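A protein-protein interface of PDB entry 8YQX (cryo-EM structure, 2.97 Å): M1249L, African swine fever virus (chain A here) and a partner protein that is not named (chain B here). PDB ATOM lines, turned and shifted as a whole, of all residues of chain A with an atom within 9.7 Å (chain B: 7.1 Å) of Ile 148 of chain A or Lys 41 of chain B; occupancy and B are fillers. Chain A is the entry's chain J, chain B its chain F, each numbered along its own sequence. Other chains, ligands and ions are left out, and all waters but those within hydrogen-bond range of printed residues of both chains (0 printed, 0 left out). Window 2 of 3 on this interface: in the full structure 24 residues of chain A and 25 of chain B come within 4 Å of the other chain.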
ATOM      1  N   GLN A 140      27.111  26.612  -5.575  1.00  0.00           N
ATOM      2  CA  GLN A 140      28.248  25.716  -5.732  1.00  0.00           C
ATOM      3  C   GLN A 140      28.018  24.369  -5.062  1.00  0.00           C
ATOM      4  O   GLN A 140      28.520  23.356  -5.555  1.00  0.00           O
ATOM      5  CB  GLN A 140      29.515  26.368  -5.174  1.00  0.00           C
ATOM      6  CG  GLN A 140      30.040  27.516  -6.020  1.00  0.00           C
ATOM      7  CD  GLN A 140      29.596  28.869  -5.506  1.00  0.00           C
ATOM      8  OE1 GLN A 140      29.305  29.031  -4.322  1.00  0.00           O
ATOM      9  NE2 GLN A 140      29.536  29.851  -6.398  1.00  0.00           N
ATOM     10  N   CYS A 141      27.273  24.329  -3.955  1.00  0.00           N
ATOM     11  CA  CYS A 141      26.935  23.048  -3.343  1.00  0.00           C
ATOM     12  C   CYS A 141      26.075  22.198  -4.270  1.00  0.00           C
ATOM     13  O   CYS A 141      26.318  20.993  -4.416  1.00  0.00           O
ATOM     14  CB  CYS A 141      26.219  23.276  -2.011  1.00  0.00           C
ATOM     15  SG  CYS A 141      25.666  21.761  -1.193  1.00  0.00           S
ATOM     16  N   PHE A 142      25.075  22.807  -4.909  1.00  0.00           N
ATOM     17  CA  PHE A 142      24.260  22.069  -5.868  1.00  0.00           C
ATOM     18  C   PHE A 142      25.086  21.648  -7.076  1.00  0.00           C
ATOM     19  O   PHE A 142      24.889  20.555  -7.621  1.00  0.00           O
ATOM     20  CB  PHE A 142      23.062  22.910  -6.304  1.00  0.00           C
ATOM     21  CG  PHE A 142      22.061  22.150  -7.124  1.00  0.00           C
ATOM     22  CD1 PHE A 142      21.139  21.319  -6.514  1.00  0.00           C
ATOM     23  CD2 PHE A 142      22.046  22.261  -8.503  1.00  0.00           C
ATOM     24  CE1 PHE A 142      20.218  20.616  -7.264  1.00  0.00           C
ATOM     25  CE2 PHE A 142      21.129  21.560  -9.258  1.00  0.00           C
ATOM     26  CZ  PHE A 142      20.214  20.737  -8.637  1.00  0.00           C
ATOM     27  N   MET A 143      26.015  22.503  -7.510  1.00  0.00           N
ATOM     28  CA  MET A 143      26.910  22.136  -8.603  1.00  0.00           C
ATOM     29  C   MET A 143      27.745  20.917  -8.241  1.00  0.00           C
ATOM     30  O   MET A 143      27.895  19.992  -9.045  1.00  0.00           O
ATOM     31  CB  MET A 143      27.811  23.318  -8.960  1.00  0.00           C
ATOM     32  CG  MET A 143      27.116  24.403  -9.751  1.00  0.00           C
ATOM     33  SD  MET A 143      25.592  23.804 -10.496  1.00  0.00           S
ATOM     34  CE  MET A 143      26.211  23.142 -12.042  1.00  0.00           C
ATOM     35  N   ARG A 144      28.290  20.895  -7.025  1.00  0.00           N
ATOM     36  CA  ARG A 144      29.092  19.758  -6.586  1.00  0.00           C
ATOM     37  C   ARG A 144      28.251  18.491  -6.495  1.00  0.00           C
ATOM     38  O   ARG A 144      28.692  17.410  -6.908  1.00  0.00           O
ATOM     39  CB  ARG A 144      29.737  20.074  -5.237  1.00  0.00           C
ATOM     40  CG  ARG A 144      31.095  19.438  -5.025  1.00  0.00           C
ATOM     41  CD  ARG A 144      31.681  19.862  -3.689  1.00  0.00           C
ATOM     42  NE  ARG A 144      33.054  19.404  -3.517  1.00  0.00           N
ATOM     43  CZ  ARG A 144      33.713  19.442  -2.369  1.00  0.00           C
ATOM     44  NH1 ARG A 144      33.153  19.908  -1.265  1.00  0.00           N
ATOM     45  NH2 ARG A 144      34.967  19.000  -2.326  1.00  0.00           N
ATOM     46  N   MET A 145      27.033  18.603  -5.961  1.00  0.00           N
ATOM     47  CA  MET A 145      26.186  17.423  -5.818  1.00  0.00           C
ATOM     48  C   MET A 145      25.722  16.891  -7.168  1.00  0.00           C
ATOM     49  O   MET A 145      25.563  15.675  -7.329  1.00  0.00           O
ATOM     50  CB  MET A 145      24.992  17.740  -4.921  1.00  0.00           C
ATOM     51  CG  MET A 145      25.375  18.003  -3.477  1.00  0.00           C
ATOM     52  SD  MET A 145      23.963  18.318  -2.409  1.00  0.00           S
ATOM     53  CE  MET A 145      22.709  17.309  -3.191  1.00  0.00           C
ATOM     54  N   ALA A 146      25.489  17.773  -8.143  1.00  0.00           N
ATOM     55  CA  ALA A 146      25.175  17.310  -9.489  1.00  0.00           C
ATOM     56  C   ALA A 146      26.406  16.738 -10.179  1.00  0.00           C
ATOM     57  O   ALA A 146      26.286  15.836 -11.015  1.00  0.00           O
ATOM     58  CB  ALA A 146      24.580  18.450 -10.315  1.00  0.00           C
ATOM     59  N   GLU A 147      27.592  17.255  -9.846  1.00  0.00           N
ATOM     60  CA  GLU A 147      28.831  16.678 -10.355  1.00  0.00           C
ATOM     61  C   GLU A 147      29.014  15.252  -9.859  1.00  0.00           C
ATOM     62  O   GLU A 147      29.458  14.377 -10.612  1.00  0.00           O
ATOM     63  CB  GLU A 147      30.029  17.537  -9.945  1.00  0.00           C
ATOM     64  CG  GLU A 147      30.060  18.911 -10.596  1.00  0.00           C
ATOM     65  CD  GLU A 147      31.221  19.758 -10.110  1.00  0.00           C
ATOM     66  OE1 GLU A 147      31.886  19.354  -9.134  1.00  0.00           O
ATOM     67  OE2 GLU A 147      31.466  20.830 -10.704  1.00  0.00           O
ATOM     68  N   ILE A 148      28.693  15.002  -8.588  1.00  0.00           N
ATOM     69  CA  ILE A 148      28.744  13.638  -8.067  1.00  0.00           C
ATOM     70  C   ILE A 148      27.738  12.757  -8.800  1.00  0.00           C
ATOM     71  O   ILE A 148      28.075  11.674  -9.291  1.00  0.00           O
ATOM     72  CB  ILE A 148      28.505  13.636  -6.547  1.00  0.00           C
ATOM     73  CG1 ILE A 148      29.764  14.110  -5.818  1.00  0.00           C
ATOM     74  CG2 ILE A 148      28.097  12.254  -6.070  1.00  0.00           C
ATOM     75  CD1 ILE A 148      29.542  14.439  -4.362  1.00  0.00           C
ATOM     76  N   GLY A 149      26.491  13.215  -8.892  1.00  0.00           N
ATOM     77  CA  GLY A 149      25.506  12.609  -9.763  1.00  0.00           C
ATOM     78  C   GLY A 149      24.742  11.436  -9.190  1.00  0.00           C
ATOM     79  O   GLY A 149      23.785  10.978  -9.824  1.00  0.00           O
ATOM     80  N   SER A 150      25.121  10.935  -8.018  1.00  0.00           N
ATOM     81  CA  SER A 150      24.470   9.771  -7.431  1.00  0.00           C
ATOM     82  C   SER A 150      23.449  10.129  -6.362  1.00  0.00           C
ATOM     83  O   SER A 150      22.874   9.223  -5.750  1.00  0.00           O
ATOM     84  CB  SER A 150      25.518   8.824  -6.842  1.00  0.00           C
ATOM     85  OG  SER A 150      26.272   9.469  -5.832  1.00  0.00           O
ATOM     86  N   PHE A 151      23.207  11.413  -6.123  1.00  0.00           N
ATOM     87  CA  PHE A 151      22.328  11.827  -5.040  1.00  0.00           C
ATOM     88  C   PHE A 151      20.864  11.602  -5.398  1.00  0.00           C
ATOM     89  O   PHE A 151      20.469  11.641  -6.567  1.00  0.00           O
ATOM     90  CB  PHE A 151      22.563  13.297  -4.695  1.00  0.00           C
ATOM     91  CG  PHE A 151      23.759  13.526  -3.823  1.00  0.00           C
ATOM     92  CD1 PHE A 151      23.675  13.359  -2.452  1.00  0.00           C
ATOM     93  CD2 PHE A 151      24.972  13.901  -4.372  1.00  0.00           C
ATOM     94  CE1 PHE A 151      24.776  13.566  -1.646  1.00  0.00           C
ATOM     95  CE2 PHE A 151      26.076  14.111  -3.571  1.00  0.00           C
ATOM     96  CZ  PHE A 151      25.978  13.942  -2.206  1.00  0.00           C
ATOM     97  N   SER A 152      20.060  11.358  -4.367  1.00  0.00           N
ATOM     98  CA  SER A 152      18.635  11.150  -4.553  1.00  0.00           C
ATOM     99  C   SER A 152      17.947  12.469  -4.900  1.00  0.00           C
ATOM    100  O   SER A 152      18.425  13.544  -4.531  1.00  0.00           O
ATOM    101  CB  SER A 152      18.020  10.557  -3.288  1.00  0.00           C
ATOM    102  OG  SER A 152      16.620  10.388  -3.417  1.00  0.00           O
ATOM    103  N   PRO A 153      16.827  12.414  -5.627  1.00  0.00           N
ATOM    104  CA  PRO A 153      16.072  13.650  -5.892  1.00  0.00           C
ATOM    105  C   PRO A 153      15.601  14.358  -4.635  1.00  0.00           C
ATOM    106  O   PRO A 153      15.492  15.589  -4.637  1.00  0.00           O
ATOM    107  CB  PRO A 153      14.890  13.158  -6.740  1.00  0.00           C
ATOM    108  CG  PRO A 153      15.397  11.926  -7.400  1.00  0.00           C
ATOM    109  CD  PRO A 153      16.312  11.274  -6.405  1.00  0.00           C
ATOM    110  N   LEU A 156      18.631  16.424  -3.665  1.00  0.00           N
ATOM    111  CA  LEU A 156      18.923  17.434  -4.677  1.00  0.00           C
ATOM    112  C   LEU A 156      17.918  18.574  -4.616  1.00  0.00           C
ATOM    113  O   LEU A 156      18.293  19.750  -4.663  1.00  0.00           O
ATOM    114  CB  LEU A 156      18.927  16.797  -6.067  1.00  0.00           C
ATOM    115  CG  LEU A 156      20.199  16.075  -6.514  1.00  0.00           C
ATOM    116  CD1 LEU A 156      19.970  15.398  -7.851  1.00  0.00           C
ATOM    117  CD2 LEU A 156      21.361  17.048  -6.600  1.00  0.00           C
ATOM    118  N   ASN A 220      16.034  16.602 -11.777  1.00  0.00           N
ATOM    119  CA  ASN A 220      16.981  15.954 -12.677  1.00  0.00           C
ATOM    120  C   ASN A 220      17.180  16.776 -13.942  1.00  0.00           C
ATOM    121  O   ASN A 220      18.311  16.936 -14.415  1.00  0.00           O
ATOM    122  CB  ASN A 220      16.500  14.544 -13.017  1.00  0.00           C
ATOM    123  CG  ASN A 220      16.590  13.598 -11.836  1.00  0.00           C
ATOM    124  OD1 ASN A 220      17.492  13.708 -11.005  1.00  0.00           O
ATOM    125  ND2 ASN A 220      15.652  12.661 -11.754  1.00  0.00           N
ATOM    126  N   ALA A 223      19.278  19.896 -12.952  1.00  0.00           N
ATOM    127  CA  ALA A 223      20.638  19.507 -12.597  1.00  0.00           C
ATOM    128  C   ALA A 223      21.438  19.110 -13.829  1.00  0.00           C
ATOM    129  O   ALA A 223      22.616  19.464 -13.953  1.00  0.00           O
ATOM    130  CB  ALA A 223      20.611  18.365 -11.583  1.00  0.00           C
ATOM    131  N   VAL A 227      24.542  21.763 -15.383  1.00  0.00           N
ATOM    132  CA  VAL A 227      25.880  21.206 -15.573  1.00  0.00           C
ATOM    133  C   VAL A 227      26.270  21.245 -17.045  1.00  0.00           C
ATOM    134  O   VAL A 227      27.412  21.573 -17.392  1.00  0.00           O
ATOM    135  CB  VAL A 227      25.949  19.775 -15.006  1.00  0.00           C
ATOM    136  CG1 VAL A 227      27.248  19.102 -15.412  1.00  0.00           C
ATOM    137  CG2 VAL A 227      25.817  19.799 -13.497  1.00  0.00           C
ATOM    138  N   LYS A 230      27.199  24.763 -17.902  1.00  0.00           N
ATOM    139  CA  LYS A 230      28.514  25.092 -17.360  1.00  0.00           C
ATOM    140  C   LYS A 230      29.625  24.496 -18.215  1.00  0.00           C
ATOM    141  O   LYS A 230      30.623  25.165 -18.511  1.00  0.00           O
ATOM    142  CB  LYS A 230      28.619  24.610 -15.911  1.00  0.00           C
ATOM    143  CG  LYS A 230      29.924  23.908 -15.566  1.00  0.00           C
ATOM    144  CD  LYS A 230      29.917  23.395 -14.137  1.00  0.00           C
ATOM    145  CE  LYS A 230      31.223  22.702 -13.794  1.00  0.00           C
ATOM    146  NZ  LYS A 230      31.398  21.442 -14.567  1.00  0.00           N
ATOM    147  N   LYS B   5      21.233  12.224 -18.648  1.00  0.00           N
ATOM    148  CA  LYS B   5      22.059  12.381 -17.460  1.00  0.00           C
ATOM    149  C   LYS B   5      23.508  12.492 -17.902  1.00  0.00           C
ATOM    150  O   LYS B   5      23.864  12.099 -19.013  1.00  0.00           O
ATOM    151  CB  LYS B   5      21.866  11.216 -16.485  1.00  0.00           C
ATOM    152  CG  LYS B   5      22.233  11.538 -15.048  1.00  0.00           C
ATOM    153  CD  LYS B   5      21.911  10.379 -14.125  1.00  0.00           C
ATOM    154  CE  LYS B   5      22.340  10.677 -12.704  1.00  0.00           C
ATOM    155  NZ  LYS B   5      23.785  11.021 -12.630  1.00  0.00           N
ATOM    156  N   ILE B   6      24.339  13.049 -17.025  1.00  0.00           N
ATOM    157  CA  ILE B   6      25.762  13.222 -17.289  1.00  0.00           C
ATOM    158  C   ILE B   6      26.542  12.525 -16.186  1.00  0.00           C
ATOM    159  O   ILE B   6      26.320  12.790 -14.999  1.00  0.00           O
ATOM    160  CB  ILE B   6      26.147  14.709 -17.383  1.00  0.00           C
ATOM    161  CG1 ILE B   6      25.427  15.367 -18.560  1.00  0.00           C
ATOM    162  CG2 ILE B   6      27.648  14.862 -17.535  1.00  0.00           C
ATOM    163  CD1 ILE B   6      25.700  16.844 -18.692  1.00  0.00           C
ATOM    164  N   PHE B   7      27.454  11.640 -16.578  1.00  0.00           N
ATOM    165  CA  PHE B   7      28.238  10.843 -15.649  1.00  0.00           C
ATOM    166  C   PHE B   7      29.717  11.165 -15.802  1.00  0.00           C
ATOM    167  O   PHE B   7      30.171  11.595 -16.866  1.00  0.00           O
ATOM    168  CB  PHE B   7      28.040   9.340 -15.885  1.00  0.00           C
ATOM    169  CG  PHE B   7      26.626   8.868 -15.718  1.00  0.00           C
ATOM    170  CD1 PHE B   7      25.708   9.015 -16.742  1.00  0.00           C
ATOM    171  CD2 PHE B   7      26.224   8.251 -14.550  1.00  0.00           C
ATOM    172  CE1 PHE B   7      24.413   8.573 -16.595  1.00  0.00           C
ATOM    173  CE2 PHE B   7      24.928   7.806 -14.398  1.00  0.00           C
ATOM    174  CZ  PHE B   7      24.024   7.965 -15.423  1.00  0.00           C
ATOM    175  N   GLU B   8      30.461  10.943 -14.722  1.00  0.00           N
ATOM    176  CA  GLU B   8      31.915  10.962 -14.730  1.00  0.00           C
ATOM    177  C   GLU B   8      32.429   9.561 -14.431  1.00  0.00           C
ATOM    178  O   GLU B   8      31.848   8.841 -13.614  1.00  0.00           O
ATOM    179  CB  GLU B   8      32.472  11.937 -13.692  1.00  0.00           C
ATOM    180  CG  GLU B   8      32.399  13.396 -14.075  1.00  0.00           C
ATOM    181  CD  GLU B   8      33.014  14.289 -13.017  1.00  0.00           C
ATOM    182  OE1 GLU B   8      33.233  13.803 -11.888  1.00  0.00           O
ATOM    183  OE2 GLU B   8      33.287  15.469 -13.313  1.00  0.00           O
ATOM    184  N   THR B   9      33.517   9.176 -15.088  1.00  0.00           N
ATOM    185  CA  THR B   9      34.097   7.861 -14.858  1.00  0.00           C
ATOM    186  C   THR B   9      35.566   7.900 -15.249  1.00  0.00           C
ATOM    187  O   THR B   9      36.036   8.851 -15.873  1.00  0.00           O
ATOM    188  CB  THR B   9      33.351   6.776 -15.640  1.00  0.00           C
ATOM    189  OG1 THR B   9      33.802   5.484 -15.218  1.00  0.00           O
ATOM    190  CG2 THR B   9      33.595   6.932 -17.129  1.00  0.00           C
ATOM    191  N   LYS B  38      23.234  -1.338 -17.231  1.00  0.00           N
ATOM    192  CA  LYS B  38      23.532  -1.572 -15.827  1.00  0.00           C
ATOM    193  C   LYS B  38      23.154  -0.347 -15.007  1.00  0.00           C
ATOM    194  O   LYS B  38      23.113   0.776 -15.512  1.00  0.00           O
ATOM    195  CB  LYS B  38      25.015  -1.906 -15.618  1.00  0.00           C
ATOM    196  CG  LYS B  38      25.460  -3.188 -16.298  1.00  0.00           C
ATOM    197  CD  LYS B  38      26.968  -3.343 -16.242  1.00  0.00           C
ATOM    198  CE  LYS B  38      27.437  -4.470 -17.143  1.00  0.00           C
ATOM    199  NZ  LYS B  38      27.239  -4.144 -18.580  1.00  0.00           N
ATOM    200  N   CYS B  39      22.873  -0.583 -13.728  1.00  0.00           N
ATOM    201  CA  CYS B  39      22.563   0.487 -12.792  1.00  0.00           C
ATOM    202  C   CYS B  39      23.857   1.106 -12.282  1.00  0.00           C
ATOM    203  O   CYS B  39      24.791   0.388 -11.913  1.00  0.00           O
ATOM    204  CB  CYS B  39      21.732  -0.038 -11.623  1.00  0.00           C
ATOM    205  SG  CYS B  39      20.062  -0.546 -12.061  1.00  0.00           S
ATOM    206  N   PHE B  40      23.909   2.436 -12.264  1.00  0.00           N
ATOM    207  CA  PHE B  40      25.103   3.142 -11.820  1.00  0.00           C
ATOM    208  C   PHE B  40      24.712   4.557 -11.428  1.00  0.00           C
ATOM    209  O   PHE B  40      24.106   5.276 -12.227  1.00  0.00           O
ATOM    210  CB  PHE B  40      26.171   3.160 -12.919  1.00  0.00           C
ATOM    211  CG  PHE B  40      27.412   3.922 -12.554  1.00  0.00           C
ATOM    212  CD1 PHE B  40      28.187   3.534 -11.475  1.00  0.00           C
ATOM    213  CD2 PHE B  40      27.811   5.017 -13.299  1.00  0.00           C
ATOM    214  CE1 PHE B  40      29.332   4.230 -11.141  1.00  0.00           C
ATOM    215  CE2 PHE B  40      28.955   5.717 -12.968  1.00  0.00           C
ATOM    216  CZ  PHE B  40      29.716   5.322 -11.888  1.00  0.00           C
ATOM    217  N   LYS B  41      25.053   4.943 -10.198  1.00  0.00           N
ATOM    218  CA  LYS B  41      24.773   6.274  -9.664  1.00  0.00           C
ATOM    219  C   LYS B  41      23.274   6.585  -9.703  1.00  0.00           C
ATOM    220  O   LYS B  41      22.824   7.555 -10.316  1.00  0.00           O
ATOM    221  CB  LYS B  41      25.583   7.343 -10.404  1.00  0.00           C
ATOM    222  CG  LYS B  41      27.026   7.438  -9.947  1.00  0.00           C
ATOM    223  CD  LYS B  41      27.796   8.467 -10.748  1.00  0.00           C
ATOM    224  CE  LYS B  41      29.228   8.581 -10.258  1.00  0.00           C
ATOM    225  NZ  LYS B  41      29.971   9.659 -10.967  1.00  0.00           N
ATOM    226  N   ASN B  42      22.506   5.724  -9.033  1.00  0.00           N
ATOM    227  CA  ASN B  42      21.077   5.938  -8.794  1.00  0.00           C
ATOM    228  C   ASN B  42      20.279   6.040 -10.091  1.00  0.00           C
ATOM    229  O   ASN B  42      19.229   6.685 -10.134  1.00  0.00           O
ATOM    230  CB  ASN B  42      20.843   7.179  -7.929  1.00  0.00           C
ATOM    231  CG  ASN B  42      19.726   6.989  -6.925  1.00  0.00           C
ATOM    232  OD1 ASN B  42      19.295   5.867  -6.663  1.00  0.00           O
ATOM    233  ND2 ASN B  42      19.246   8.089  -6.361  1.00  0.00           N
ATOM    234  N   SER B  43      20.758   5.405 -11.157  1.00  0.00           N
ATOM    235  CA  SER B  43      20.037   5.413 -12.421  1.00  0.00           C
ATOM    236  C   SER B  43      20.441   4.189 -13.227  1.00  0.00           C
ATOM    237  O   SER B  43      21.499   3.598 -13.004  1.00  0.00           O
ATOM    238  CB  SER B  43      20.303   6.695 -13.215  1.00  0.00           C
ATOM    239  OG  SER B  43      21.667   6.791 -13.583  1.00  0.00           O
ATOM    240  N   PHE B  44      19.580   3.822 -14.172  1.00  0.00           N
ATOM    241  CA  PHE B  44      19.815   2.700 -15.071  1.00  0.00           C
ATOM    242  C   PHE B  44      20.142   3.248 -16.453  1.00  0.00           C
ATOM    243  O   PHE B  44      19.287   3.867 -17.095  1.00  0.00           O
ATOM    244  CB  PHE B  44      18.595   1.780 -15.128  1.00  0.00           C
ATOM    245  CG  PHE B  44      18.798   0.559 -15.975  1.00  0.00           C
ATOM    246  CD1 PHE B  44      19.405  -0.568 -15.454  1.00  0.00           C
ATOM    247  CD2 PHE B  44      18.382   0.539 -17.293  1.00  0.00           C
ATOM    248  CE1 PHE B  44      19.592  -1.689 -16.230  1.00  0.00           C
ATOM    249  CE2 PHE B  44      18.569  -0.579 -18.074  1.00  0.00           C
ATOM    250  CZ  PHE B  44      19.172  -1.695 -17.542  1.00  0.00           C
ATOM    251  N   ILE B  45      21.367   3.011 -16.911  1.00  0.00           N
ATOM    252  CA  ILE B  45      21.830   3.564 -18.179  1.00  0.00           C
ATOM    253  C   ILE B  45      21.234   2.755 -19.323  1.00  0.00           C
ATOM    254  O   ILE B  45      21.434   1.540 -19.409  1.00  0.00           O
ATOM    255  CB  ILE B  45      23.363   3.575 -18.254  1.00  0.00           C
ATOM    256  CG1 ILE B  45      23.945   4.513 -17.198  1.00  0.00           C
ATOM    257  CG2 ILE B  45      23.823   3.995 -19.636  1.00  0.00           C
ATOM    258  CD1 ILE B  45      24.675   3.801 -16.096  1.00  0.00           C
ATOM    259  N   TYR B  80      14.674   6.473 -14.751  1.00  0.00           N
ATOM    260  CA  TYR B  80      14.482   6.494 -13.307  1.00  0.00           C
ATOM    261  C   TYR B  80      13.010   6.262 -13.016  1.00  0.00           C
ATOM    262  O   TYR B  80      12.149   6.943 -13.581  1.00  0.00           O
ATOM    263  CB  TYR B  80      14.954   7.821 -12.707  1.00  0.00           C
ATOM    264  CG  TYR B  80      14.955   7.845 -11.196  1.00  0.00           C
ATOM    265  CD1 TYR B  80      13.882   8.365 -10.487  1.00  0.00           C
ATOM    266  CD2 TYR B  80      16.033   7.345 -10.478  1.00  0.00           C
ATOM    267  CE1 TYR B  80      13.882   8.387  -9.107  1.00  0.00           C
ATOM    268  CE2 TYR B  80      16.041   7.363  -9.097  1.00  0.00           C
ATOM    269  CZ  TYR B  80      14.962   7.885  -8.418  1.00  0.00           C
ATOM    270  OH  TYR B  80      14.965   7.904  -7.042  1.00  0.00           O
ATOM    271  N   TYR B 141      18.468   1.101  -7.031  1.00  0.00           N
ATOM    272  CA  TYR B 141      19.326   0.924  -8.198  1.00  0.00           C
ATOM    273  C   TYR B 141      20.688   0.464  -7.686  1.00  0.00           C
ATOM    274  O   TYR B 141      21.596   1.269  -7.478  1.00  0.00           O
ATOM    275  CB  TYR B 141      19.423   2.214  -9.006  1.00  0.00           C
ATOM    276  CG  TYR B 141      18.161   2.547  -9.765  1.00  0.00           C
ATOM    277  CD1 TYR B 141      17.820   1.857 -10.918  1.00  0.00           C
ATOM    278  CD2 TYR B 141      17.306   3.547  -9.327  1.00  0.00           C
ATOM    279  CE1 TYR B 141      16.668   2.154 -11.615  1.00  0.00           C
ATOM    280  CE2 TYR B 141      16.150   3.851 -10.017  1.00  0.00           C
ATOM    281  CZ  TYR B 141      15.837   3.150 -11.160  1.00  0.00           C
ATOM    282  OH  TYR B 141      14.687   3.446 -11.854  1.00  0.00           O
ATOM    283  N   ILE B 142      20.821  -0.840  -7.490  1.00  0.00           N
ATOM    284  CA  ILE B 142      22.073  -1.402  -6.971  1.00  0.00           C
ATOM    285  C   ILE B 142      23.117  -1.397  -8.081  1.00  0.00           C
ATOM    286  O   ILE B 142      22.847  -1.908  -9.182  1.00  0.00           O
ATOM    287  CB  ILE B 142      21.839  -2.814  -6.437  1.00  0.00           C
ATOM    288  CG1 ILE B 142      21.046  -2.759  -5.131  1.00  0.00           C
ATOM    289  CG2 ILE B 142      23.161  -3.523  -6.211  1.00  0.00           C
ATOM    290  CD1 ILE B 142      19.708  -3.455  -5.201  1.00  0.00           C
ATOM    291  N   PRO B 143      24.303  -0.834  -7.853  1.00  0.00           N
ATOM    292  CA  PRO B 143      25.304  -0.749  -8.924  1.00  0.00           C
ATOM    293  C   PRO B 143      25.686  -2.124  -9.453  1.00  0.00           C
ATOM    294  O   PRO B 143      25.834  -3.084  -8.693  1.00  0.00           O
ATOM    295  CB  PRO B 143      26.489  -0.057  -8.242  1.00  0.00           C
ATOM    296  CG  PRO B 143      25.885   0.689  -7.103  1.00  0.00           C
ATOM    297  CD  PRO B 143      24.754  -0.165  -6.622  1.00  0.00           C
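Ile 148 of chain A touches just one residue of chain B: Lys 41. Printed residues of chain B within 4 Å of Ser 150 of chain A: Lys 41 (3.7 Å) and Asn 42 (3.6 Å). Of the printed residues of chain B, Phe 151 of chain A touches Asn 42 (3.8 Å). Printed residues of chain B within 4 Å of Pro 153 of chain A: Tyr 80. Of the printed residues of chain A, Lys 5 of chain B touches Gly 149. Of chain A, only Ile 148, Gly 149 and Ser 150 come within 4 Å of Lys 41 of chain B. Printed residues of chain A within 4 Å of Asn 42 of chain B: Ser 150, Phe 151 and Ser 152. No residue of chain A comes within 4 Å of Ser 43 of chain B. The nearest residue of chain B that does not touch Ile 148 of chain A is Lys 5 of chain B (5.5 Å). The nearest printed residue of chain B that does not touch Phe 151 of chain A is Lys 41 of chain B (5.7 Å).
NZ of Lys 41 of chain B sits at hydrogen-bond distance from O of Glu 8 of chain B (3.3 Å).
NZ of Lys 5 of chain B is in hydrogen-bond range of O of Gly 149 of chain A, 2.8 Å away. The side-chain amino group (NZ) of Lys 41 of chain B is in hydrogen-bond range of the backbone carbonyl oxygen (O) of Ile 148 of chain A (3.2 Å).
Hydrophobic or aromatic side chains of chain B within 4 Å of the printed part of chain A: Tyr 80. Along chain B the printed residues that touch a printed residue of chain A span positions 5 to 80. Among the printed residues, 8 pairs touch across the chains.
O of Gly 149 of chain A touches O of Lys 41 of chain B, 3.6 Å away. Lys 41 of chain B touches Ser 150 of chain A (CG to CB, 3.7 Å). Ser 150 of chain A touches Asn 42 of chain B (O to CB, 3.6 Å). ND2 of Asn 42 of chain B touches O of Phe 151 of chain A (3.8 Å). Ser 152 of chain A touches Asn 42 of chain B. Pro 153 of chain A touches Tyr 80 of chain B.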
